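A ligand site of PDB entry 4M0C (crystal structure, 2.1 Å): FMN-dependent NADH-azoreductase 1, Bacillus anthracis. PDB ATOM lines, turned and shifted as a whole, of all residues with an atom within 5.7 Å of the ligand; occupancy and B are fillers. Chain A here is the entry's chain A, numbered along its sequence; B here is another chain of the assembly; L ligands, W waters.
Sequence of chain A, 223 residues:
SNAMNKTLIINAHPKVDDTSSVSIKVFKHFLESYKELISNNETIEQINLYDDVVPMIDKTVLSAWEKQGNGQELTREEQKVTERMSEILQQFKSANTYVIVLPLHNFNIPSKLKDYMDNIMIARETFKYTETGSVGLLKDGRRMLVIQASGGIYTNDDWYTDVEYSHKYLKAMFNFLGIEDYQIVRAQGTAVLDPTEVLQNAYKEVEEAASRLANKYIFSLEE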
ATOM      1  N   HIS A  13     -22.691  14.540  17.121  1.00  0.00           N
ATOM      2  CA  HIS A  13     -23.976  13.965  16.759  1.00  0.00           C
ATOM      3  C   HIS A  13     -24.700  13.464  17.993  1.00  0.00           C
ATOM      4  O   HIS A  13     -24.143  12.695  18.781  1.00  0.00           O
ATOM      5  CB  HIS A  13     -23.829  12.827  15.741  1.00  0.00           C
ATOM      6  CG  HIS A  13     -25.103  12.502  15.016  1.00  0.00           C
ATOM      7  ND1 HIS A  13     -26.216  11.980  15.652  1.00  0.00           N
ATOM      8  CD2 HIS A  13     -25.459  12.658  13.719  1.00  0.00           C
ATOM      9  CE1 HIS A  13     -27.187  11.825  14.775  1.00  0.00           C
ATOM     10  NE2 HIS A  13     -26.746  12.209  13.593  1.00  0.00           N
ATOM     11  N   LYS A  15     -26.928  11.268  18.421  1.00  0.00           N
ATOM     12  CA  LYS A  15     -27.077   9.814  18.521  1.00  0.00           C
ATOM     13  C   LYS A  15     -25.770   9.118  18.881  1.00  0.00           C
ATOM     14  O   LYS A  15     -25.751   7.907  19.107  1.00  0.00           O
ATOM     15  CB  LYS A  15     -27.644   9.231  17.209  1.00  0.00           C
ATOM     16  CG  LYS A  15     -29.048   9.719  16.860  1.00  0.00           C
ATOM     17  CD  LYS A  15     -29.660   8.889  15.727  1.00  0.00           C
ATOM     18  CE  LYS A  15     -31.116   9.284  15.470  1.00  0.00           C
ATOM     19  NZ  LYS A  15     -31.753   8.452  14.430  1.00  0.00           N
ATOM     20  N   SER A  20     -27.499   4.192  12.176  1.00  0.00           N
ATOM     21  CA  SER A  20     -28.610   4.612  11.324  1.00  0.00           C
ATOM     22  C   SER A  20     -28.317   5.997  10.719  1.00  0.00           C
ATOM     23  O   SER A  20     -28.802   6.315   9.634  1.00  0.00           O
ATOM     24  CB  SER A  20     -29.934   4.606  12.094  1.00  0.00           C
ATOM     25  OG  SER A  20     -29.968   5.591  13.115  1.00  0.00           O
ATOM     26  N   SER A  21     -27.481   6.771  11.408  1.00  0.00           N
ATOM     27  CA  SER A  21     -27.121   8.134  10.995  1.00  0.00           C
ATOM     28  C   SER A  21     -26.142   8.184   9.799  1.00  0.00           C
ATOM     29  O   SER A  21     -25.120   7.477   9.795  1.00  0.00           O
ATOM     30  CB  SER A  21     -26.488   8.840  12.190  1.00  0.00           C
ATOM     31  OG  SER A  21     -25.603   9.883  11.786  1.00  0.00           O
ATOM     32  N   VAL A  22     -26.413   9.038   8.809  1.00  0.00           N
ATOM     33  CA  VAL A  22     -25.527   9.150   7.643  1.00  0.00           C
ATOM     34  C   VAL A  22     -24.139   9.624   8.055  1.00  0.00           C
ATOM     35  O   VAL A  22     -23.141   9.037   7.666  1.00  0.00           O
ATOM     36  CB  VAL A  22     -26.084  10.119   6.572  1.00  0.00           C
ATOM     37  CG1 VAL A  22     -25.057  10.321   5.464  1.00  0.00           C
ATOM     38  CG2 VAL A  22     -27.394   9.596   5.976  1.00  0.00           C
ATOM     39  N   SER A  23     -24.084  10.677   8.867  1.00  0.00           N
ATOM     40  CA  SER A  23     -22.790  11.263   9.221  1.00  0.00           C
ATOM     41  C   SER A  23     -21.945  10.347  10.116  1.00  0.00           C
ATOM     42  O   SER A  23     -20.718  10.323  10.005  1.00  0.00           O
ATOM     43  CB  SER A  23     -22.967  12.662   9.817  1.00  0.00           C
ATOM     44  OG  SER A  23     -23.630  12.626  11.070  1.00  0.00           O
ATOM     45  N   ILE A  24     -22.594   9.571  10.986  1.00  0.00           N
ATOM     46  CA  ILE A  24     -21.871   8.558  11.756  1.00  0.00           C
ATOM     47  C   ILE A  24     -21.332   7.398  10.870  1.00  0.00           C
ATOM     48  O   ILE A  24     -20.197   6.974  11.055  1.00  0.00           O
ATOM     49  CB  ILE A  24     -22.707   8.036  12.942  1.00  0.00           C
ATOM     50  CG1 ILE A  24     -22.959   9.158  13.944  1.00  0.00           C
ATOM     51  CG2 ILE A  24     -22.006   6.877  13.647  1.00  0.00           C
ATOM     52  CD1 ILE A  24     -24.081   8.846  14.960  1.00  0.00           C
ATOM     53  N   LEU A 102     -20.999  16.084  12.365  1.00  0.00           N
ATOM     54  CA  LEU A 102     -22.264  16.701  12.748  1.00  0.00           C
ATOM     55  C   LEU A 102     -23.357  16.451  11.716  1.00  0.00           C
ATOM     56  O   LEU A 102     -23.082  16.343  10.519  1.00  0.00           O
ATOM     57  CB  LEU A 102     -22.091  18.208  12.950  1.00  0.00           C
ATOM     58  CG  LEU A 102     -21.907  19.099  11.712  1.00  0.00           C
ATOM     59  CD1 LEU A 102     -22.232  20.547  12.037  1.00  0.00           C
ATOM     60  CD2 LEU A 102     -20.482  19.020  11.220  1.00  0.00           C
ATOM     61  N   PRO A 103     -24.599  16.342  12.191  1.00  0.00           N
ATOM     62  CA  PRO A 103     -25.762  16.435  11.288  1.00  0.00           C
ATOM     63  C   PRO A 103     -26.084  17.919  11.134  1.00  0.00           C
ATOM     64  O   PRO A 103     -25.745  18.710  12.012  1.00  0.00           O
ATOM     65  CB  PRO A 103     -26.863  15.737  12.094  1.00  0.00           C
ATOM     66  CG  PRO A 103     -26.520  16.060  13.522  1.00  0.00           C
ATOM     67  CD  PRO A 103     -25.002  16.156  13.599  1.00  0.00           C
ATOM     68  N   LEU A 104     -26.717  18.314  10.034  1.00  0.00           N
ATOM     69  CA  LEU A 104     -27.106  19.715   9.927  1.00  0.00           C
ATOM     70  C   LEU A 104     -28.530  19.829  10.408  1.00  0.00           C
ATOM     71  O   LEU A 104     -29.452  19.314   9.768  1.00  0.00           O
ATOM     72  CB  LEU A 104     -26.972  20.255   8.498  1.00  0.00           C
ATOM     73  CG  LEU A 104     -27.352  21.743   8.401  1.00  0.00           C
ATOM     74  CD1 LEU A 104     -26.507  22.623   9.345  1.00  0.00           C
ATOM     75  CD2 LEU A 104     -27.262  22.253   6.965  1.00  0.00           C
ATOM     76  N   HIS A 105     -28.710  20.505  11.537  1.00  0.00           N
ATOM     77  CA  HIS A 105     -30.042  20.752  12.073  1.00  0.00           C
ATOM     78  C   HIS A 105     -30.299  22.268  12.122  1.00  0.00           C
ATOM     79  O   HIS A 105     -29.644  22.985  12.879  1.00  0.00           O
ATOM     80  CB  HIS A 105     -30.166  20.179  13.493  1.00  0.00           C
ATOM     81  CG  HIS A 105     -30.151  18.672  13.542  1.00  0.00           C
ATOM     82  ND1 HIS A 105     -29.834  17.976  14.692  1.00  0.00           N
ATOM     83  CD2 HIS A 105     -30.439  17.747  12.598  1.00  0.00           C
ATOM     84  CE1 HIS A 105     -29.903  16.678  14.443  1.00  0.00           C
ATOM     85  NE2 HIS A 105     -30.281  16.512  13.194  1.00  0.00           N
ATOM     86  N   ASN A 106     -31.235  22.733  11.306  1.00  0.00           N
ATOM     87  CA  ASN A 106     -31.636  24.144  11.300  1.00  0.00           C
ATOM     88  C   ASN A 106     -30.489  25.121  10.996  1.00  0.00           C
ATOM     89  O   ASN A 106     -30.331  26.142  11.660  1.00  0.00           O
ATOM     90  CB  ASN A 106     -32.343  24.509  12.616  1.00  0.00           C
ATOM     91  CG  ASN A 106     -33.630  23.740  12.784  1.00  0.00           C
ATOM     92  OD1 ASN A 106     -34.485  23.738  11.889  1.00  0.00           O
ATOM     93  ND2 ASN A 106     -33.779  23.054  13.935  1.00  0.00           N
ATOM     94  N   PHE A 107     -29.678  24.750   9.994  1.00  0.00           N
ATOM     95  CA  PHE A 107     -28.756  25.688   9.339  1.00  0.00           C
ATOM     96  C   PHE A 107     -27.681  26.272  10.232  1.00  0.00           C
ATOM     97  O   PHE A 107     -27.154  27.353   9.920  1.00  0.00           O
ATOM     98  CB  PHE A 107     -29.535  26.817   8.650  1.00  0.00           C
ATOM     99  CG  PHE A 107     -30.607  26.340   7.712  1.00  0.00           C
ATOM    100  CD1 PHE A 107     -30.281  25.818   6.464  1.00  0.00           C
ATOM    101  CD2 PHE A 107     -31.942  26.406   8.066  1.00  0.00           C
ATOM    102  CE1 PHE A 107     -31.283  25.378   5.585  1.00  0.00           C
ATOM    103  CE2 PHE A 107     -32.948  25.960   7.200  1.00  0.00           C
ATOM    104  CZ  PHE A 107     -32.616  25.455   5.967  1.00  0.00           C
ATOM    105  N   ALA A 149     -23.625  15.786   7.462  1.00  0.00           N
ATOM    106  CA  ALA A 149     -24.718  15.264   6.663  1.00  0.00           C
ATOM    107  C   ALA A 149     -25.828  16.297   6.677  1.00  0.00           C
ATOM    108  O   ALA A 149     -26.049  16.966   7.679  1.00  0.00           O
ATOM    109  CB  ALA A 149     -25.221  13.938   7.225  1.00  0.00           C
ATOM    110  N   SER A 150     -26.527  16.436   5.547  1.00  0.00           N
ATOM    111  CA  SER A 150     -27.594  17.420   5.431  1.00  0.00           C
ATOM    112  C   SER A 150     -28.691  16.925   4.487  1.00  0.00           C
ATOM    113  O   SER A 150     -28.412  16.166   3.559  1.00  0.00           O
ATOM    114  CB  SER A 150     -27.011  18.750   4.920  1.00  0.00           C
ATOM    115  OG  SER A 150     -26.557  18.613   3.579  1.00  0.00           O
ATOM    116  N   GLY A 151     -29.924  17.334   4.734  1.00  0.00           N
ATOM    117  CA  GLY A 151     -31.029  16.946   3.865  1.00  0.00           C
ATOM    118  C   GLY A 151     -30.927  17.665   2.523  1.00  0.00           C
ATOM    119  O   GLY A 151     -31.203  17.075   1.470  1.00  0.00           O
ATOM    120  N   GLY A 152     -30.531  18.931   2.561  1.00  0.00           N
ATOM    121  CA  GLY A 152     -30.452  19.726   1.348  1.00  0.00           C
ATOM    122  C   GLY A 152     -29.083  19.700   0.693  1.00  0.00           C
ATOM    123  O   GLY A 152     -28.135  19.081   1.204  1.00  0.00           O
ATOM    124  N   ILE A 153     -28.961  20.385  -0.441  1.00  0.00           N
ATOM    125  CA  ILE A 153     -27.696  20.495  -1.157  1.00  0.00           C
ATOM    126  C   ILE A 153     -27.176  21.943  -1.094  1.00  0.00           C
ATOM    127  O   ILE A 153     -27.902  22.888  -1.405  1.00  0.00           O
ATOM    128  CB  ILE A 153     -27.842  20.012  -2.625  1.00  0.00           C
ATOM    129  CG1 ILE A 153     -28.169  18.507  -2.647  1.00  0.00           C
ATOM    130  CG2 ILE A 153     -26.583  20.298  -3.418  1.00  0.00           C
ATOM    131  CD1 ILE A 153     -28.689  17.994  -3.977  1.00  0.00           C
ATOM    132  N   TYR A 154     -25.912  22.108  -0.682  1.00  0.00           N
ATOM    133  CA  TYR A 154     -25.361  23.436  -0.401  1.00  0.00           C
ATOM    134  C   TYR A 154     -24.272  23.915  -1.357  1.00  0.00           C
ATOM    135  O   TYR A 154     -23.625  24.926  -1.113  1.00  0.00           O
ATOM    136  CB  TYR A 154     -24.870  23.489   1.057  1.00  0.00           C
ATOM    137  CG  TYR A 154     -26.036  23.297   1.974  1.00  0.00           C
ATOM    138  CD1 TYR A 154     -26.761  24.393   2.441  1.00  0.00           C
ATOM    139  CD2 TYR A 154     -26.459  22.029   2.337  1.00  0.00           C
ATOM    140  CE1 TYR A 154     -27.858  24.225   3.260  1.00  0.00           C
ATOM    141  CE2 TYR A 154     -27.558  21.847   3.159  1.00  0.00           C
ATOM    142  CZ  TYR A 154     -28.249  22.950   3.612  1.00  0.00           C
ATOM    143  OH  TYR A 154     -29.343  22.787   4.419  1.00  0.00           O
ATOM    144  N   TYR A 160     -29.755  28.213  -0.218  1.00  0.00           N
ATOM    145  CA  TYR A 160     -29.184  27.197   0.662  1.00  0.00           C
ATOM    146  C   TYR A 160     -27.711  27.500   0.995  1.00  0.00           C
ATOM    147  O   TYR A 160     -27.317  27.478   2.172  1.00  0.00           O
ATOM    148  CB  TYR A 160     -29.336  25.800   0.050  1.00  0.00           C
ATOM    149  CG  TYR A 160     -30.639  25.108   0.411  1.00  0.00           C
ATOM    150  CD1 TYR A 160     -30.666  24.062   1.331  1.00  0.00           C
ATOM    151  CD2 TYR A 160     -31.843  25.508  -0.162  1.00  0.00           C
ATOM    152  CE1 TYR A 160     -31.860  23.426   1.683  1.00  0.00           C
ATOM    153  CE2 TYR A 160     -33.048  24.872   0.180  1.00  0.00           C
ATOM    154  CZ  TYR A 160     -33.048  23.835   1.095  1.00  0.00           C
ATOM    155  OH  TYR A 160     -34.226  23.197   1.450  1.00  0.00           O
ATOM    156  N   ALA A 187     -22.029  15.087   3.197  1.00  0.00           N
ATOM    157  CA  ALA A 187     -22.925  14.007   2.792  1.00  0.00           C
ATOM    158  C   ALA A 187     -24.289  14.676   2.617  1.00  0.00           C
ATOM    159  O   ALA A 187     -25.155  14.573   3.506  1.00  0.00           O
ATOM    160  CB  ALA A 187     -22.974  12.924   3.863  1.00  0.00           C
ATOM    161  N   THR A 190     -29.536  14.218   1.429  1.00  0.00           N
ATOM    162  CA  THR A 190     -30.171  13.004   1.938  1.00  0.00           C
ATOM    163  C   THR A 190     -31.691  13.024   1.762  1.00  0.00           C
ATOM    164  O   THR A 190     -32.323  11.972   1.722  1.00  0.00           O
ATOM    165  CB  THR A 190     -29.796  12.702   3.418  1.00  0.00           C
ATOM    166  OG1 THR A 190     -30.247  13.758   4.281  1.00  0.00           O
ATOM    167  CG2 THR A 190     -28.279  12.547   3.560  1.00  0.00           C
ATOM    168  N   ILE B  57     -32.195  18.950  21.035  1.00  0.00           N
ATOM    169  CA  ILE B  57     -32.301  17.758  20.216  1.00  0.00           C
ATOM    170  C   ILE B  57     -31.268  16.760  20.742  1.00  0.00           C
ATOM    171  O   ILE B  57     -30.066  17.016  20.678  1.00  0.00           O
ATOM    172  CB  ILE B  57     -32.058  18.056  18.725  1.00  0.00           C
ATOM    173  CG1 ILE B  57     -33.212  18.897  18.153  1.00  0.00           C
ATOM    174  CG2 ILE B  57     -31.899  16.762  17.916  1.00  0.00           C
ATOM    175  CD1 ILE B  57     -32.897  19.488  16.792  1.00  0.00           C
ATOM    176  N   LEU B  62     -34.959  12.719  18.834  1.00  0.00           N
ATOM    177  CA  LEU B  62     -34.857  12.141  17.491  1.00  0.00           C
ATOM    178  C   LEU B  62     -35.655  10.848  17.371  1.00  0.00           C
ATOM    179  O   LEU B  62     -36.358  10.636  16.391  1.00  0.00           O
ATOM    180  CB  LEU B  62     -33.394  11.898  17.134  1.00  0.00           C
ATOM    181  CG  LEU B  62     -32.552  13.162  16.984  1.00  0.00           C
ATOM    182  CD1 LEU B  62     -31.099  12.801  16.699  1.00  0.00           C
ATOM    183  CD2 LEU B  62     -33.125  14.036  15.853  1.00  0.00           C
ATOM    184  N   TRP B  65     -39.349  11.519  17.338  1.00  0.00           N
ATOM    185  CA  TRP B  65     -39.726  12.030  16.024  1.00  0.00           C
ATOM    186  C   TRP B  65     -39.827  10.928  14.960  1.00  0.00           C
ATOM    187  O   TRP B  65     -40.730  10.964  14.122  1.00  0.00           O
ATOM    188  CB  TRP B  65     -38.745  13.116  15.574  1.00  0.00           C
ATOM    189  CG  TRP B  65     -39.005  14.431  16.244  1.00  0.00           C
ATOM    190  CD1 TRP B  65     -40.094  14.770  16.984  1.00  0.00           C
ATOM    191  CD2 TRP B  65     -38.147  15.581  16.249  1.00  0.00           C
ATOM    192  NE1 TRP B  65     -39.974  16.061  17.451  1.00  0.00           N
ATOM    193  CE2 TRP B  65     -38.785  16.573  16.999  1.00  0.00           C
ATOM    194  CE3 TRP B  65     -36.898  15.862  15.684  1.00  0.00           C
ATOM    195  CZ2 TRP B  65     -38.226  17.836  17.205  1.00  0.00           C
ATOM    196  CZ3 TRP B  65     -36.341  17.112  15.892  1.00  0.00           C
ATOM    197  CH2 TRP B  65     -37.003  18.085  16.637  1.00  0.00           C
ATOM    198  N   ASP B 118     -34.479  25.177  17.658  1.00  0.00           N
ATOM    199  CA  ASP B 118     -34.807  23.806  17.268  1.00  0.00           C
ATOM    200  C   ASP B 118     -36.210  23.402  17.699  1.00  0.00           C
ATOM    201  O   ASP B 118     -36.782  22.448  17.162  1.00  0.00           O
ATOM    202  CB  ASP B 118     -33.782  22.808  17.831  1.00  0.00           C
ATOM    203  CG  ASP B 118     -32.385  23.024  17.261  1.00  0.00           C
ATOM    204  OD1 ASP B 118     -32.267  23.613  16.153  1.00  0.00           O
ATOM    205  OD2 ASP B 118     -31.399  22.587  17.899  1.00  0.00           O
HETATM  206  N1  LIG L   1     -31.223  19.414   6.531  1.00  0.00           N
HETATM  207  C1  LIG L   1     -30.773  20.545   5.888  1.00  0.00           C
HETATM  208  O1  LIG L   1     -30.269  20.445   4.764  1.00  0.00           O
HETATM  209  N2  LIG L   1     -30.885  21.799   6.493  1.00  0.00           N
HETATM  210  C2  LIG L   1     -31.452  21.902   7.758  1.00  0.00           C
HETATM  211  O2  LIG L   1     -31.535  23.005   8.309  1.00  0.00           O
HETATM  212  C3  LIG L   1     -31.917  20.752   8.407  1.00  0.00           C
HETATM  213  N3  LIG L   1     -32.491  20.826   9.659  1.00  0.00           N
HETATM  214  C4  LIG L   1     -32.935  19.670  10.287  1.00  0.00           C
HETATM  215  C5  LIG L   1     -33.506  19.746  11.556  1.00  0.00           C
HETATM  216  C6  LIG L   1     -33.947  18.592  12.202  1.00  0.00           C
HETATM  217  C7  LIG L   1     -34.557  18.704  13.567  1.00  0.00           C
HETATM  218  C8  LIG L   1     -33.823  17.355  11.574  1.00  0.00           C
HETATM  219  C9  LIG L   1     -34.309  16.108  12.275  1.00  0.00           C
HETATM  220  C10 LIG L   1     -33.258  17.272  10.301  1.00  0.00           C
HETATM  221  C11 LIG L   1     -32.805  18.440   9.663  1.00  0.00           C
HETATM  222  N4  LIG L   1     -32.241  18.366   8.401  1.00  0.00           N
HETATM  223  C12 LIG L   1     -31.793  19.515   7.779  1.00  0.00           C
HETATM  224  C13 LIG L   1     -32.065  17.063   7.685  1.00  0.00           C
HETATM  225  C14 LIG L   1     -30.798  16.376   8.193  1.00  0.00           C
HETATM  226  O3  LIG L   1     -29.652  17.208   8.022  1.00  0.00           O
HETATM  227  C15 LIG L   1     -30.593  15.090   7.428  1.00  0.00           C
HETATM  228  O4  LIG L   1     -31.612  14.186   7.811  1.00  0.00           O
HETATM  229  C16 LIG L   1     -29.241  14.477   7.721  1.00  0.00           C
HETATM  230  O5  LIG L   1     -29.077  13.309   6.935  1.00  0.00           O
HETATM  231  C17 LIG L   1     -29.099  14.092   9.194  1.00  0.00           C
HETATM  232  O6  LIG L   1     -27.808  13.544   9.388  1.00  0.00           O
HETATM  233  P1  LIG L   1     -27.622  12.163  10.177  1.00  0.00           P
HETATM  234  O7  LIG L   1     -28.235  11.091   9.327  1.00  0.00           O
HETATM  235  O8  LIG L   1     -26.137  11.886  10.383  1.00  0.00           O
HETATM  236  O9  LIG L   1     -28.346  12.250  11.507  1.00  0.00           O
HETATM  237  O   HOH W   1     -32.835  13.771   5.228  1.00  0.00           O
HETATM  238  O   HOH W   2     -30.465  14.104  12.222  1.00  0.00           O
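N of Ser 23 sits at hydrogen-bond distance from O8 of the ligand (2.8 Å). The backbone NH (N) of Phe 107 lies within hydrogen-bond range of an oxygen (O2) of the ligand, 3.1 Å away. The backbone NH (N) of Gly 152 sits at hydrogen-bond distance from an oxygen (O1) of the ligand, at 2.7 Å. An oxygen (O5) of the ligand is in hydrogen-bond range of the side-chain hydroxyl of Thr 190, at 2.9 Å. An oxygen (O3) of the ligand is in hydrogen-bond range of the backbone carbonyl oxygen of Leu 104, at 2.7 Å. OG of Ser 21 sits at hydrogen-bond distance from O8 of the ligand (2.5 Å). A nitrogen (N1) of the ligand sits at hydrogen-bond distance from the backbone NH (N) of Gly 151 (3.0 Å). N of Asn 106 is in hydrogen-bond range of N3 of the ligand (2.8 Å). OG of Ser 23 sits at hydrogen-bond distance from O8 of the ligand (2.7 Å). The side-chain hydroxyl (OH) of Tyr 154 sits at hydrogen-bond distance from an oxygen (O1) of the ligand, 2.5 Å away. An oxygen (O9) of the ligand sits at hydrogen-bond distance from a ring nitrogen (NE2) of His 13 (2.6 Å). The backbone NH of Val 22 is in hydrogen-bond range of an oxygen (O7) of the ligand, 2.8 Å away.
O of Ala 149 is in hydrogen-bond range of N of Leu 104. The side-chain hydroxyl of Ser 21 sits at hydrogen-bond distance from the backbone NH of Ile 24 (3.1 Å). The backbone NH (N) of Lys 15 is in hydrogen-bond range of a ring nitrogen (ND1) of His 13, 2.9 Å away. The backbone carbonyl oxygen (O) of Ser 150 lies within hydrogen-bond range of the backbone NH (N) of Thr 190 (3.1 Å). The backbone NH (N) of Ala 149 is in hydrogen-bond range of the backbone carbonyl oxygen (O) of Leu 102 (3.2 Å). The side-chain hydroxyl of Ser 21 lies within hydrogen-bond range of a ring nitrogen (NE2) of His 13 (3.2 Å). ND2 of Asn 106 sits at hydrogen-bond distance from OD1 of Asp 118 of chain B, at 2.7 Å. The backbone carbonyl oxygen of Gly 152 is in hydrogen-bond range of the side-chain hydroxyl of Ser 150, 2.9 Å away.
Pro 103 touches the ligand (CB to O6, 3.6 Å). His 105 touches the ligand. Ala 149 touches the ligand (CB to O6, 3.4 Å). Ser 150 touches the ligand. Ile 57 of chain B touches the ligand (CD1 to C7, 3.7 Å). CZ3 of Trp 65 of chain B touches C7 of the ligand (3.3 Å).
Water W1 bridges the side-chain hydroxyl (OG1) of Thr 190 and an oxygen (O4) of the ligand. Water W2 bridges a ring nitrogen (NE2) of His 105 (2.6 Å) and an oxygen (O9) of the ligand (2.9 Å).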
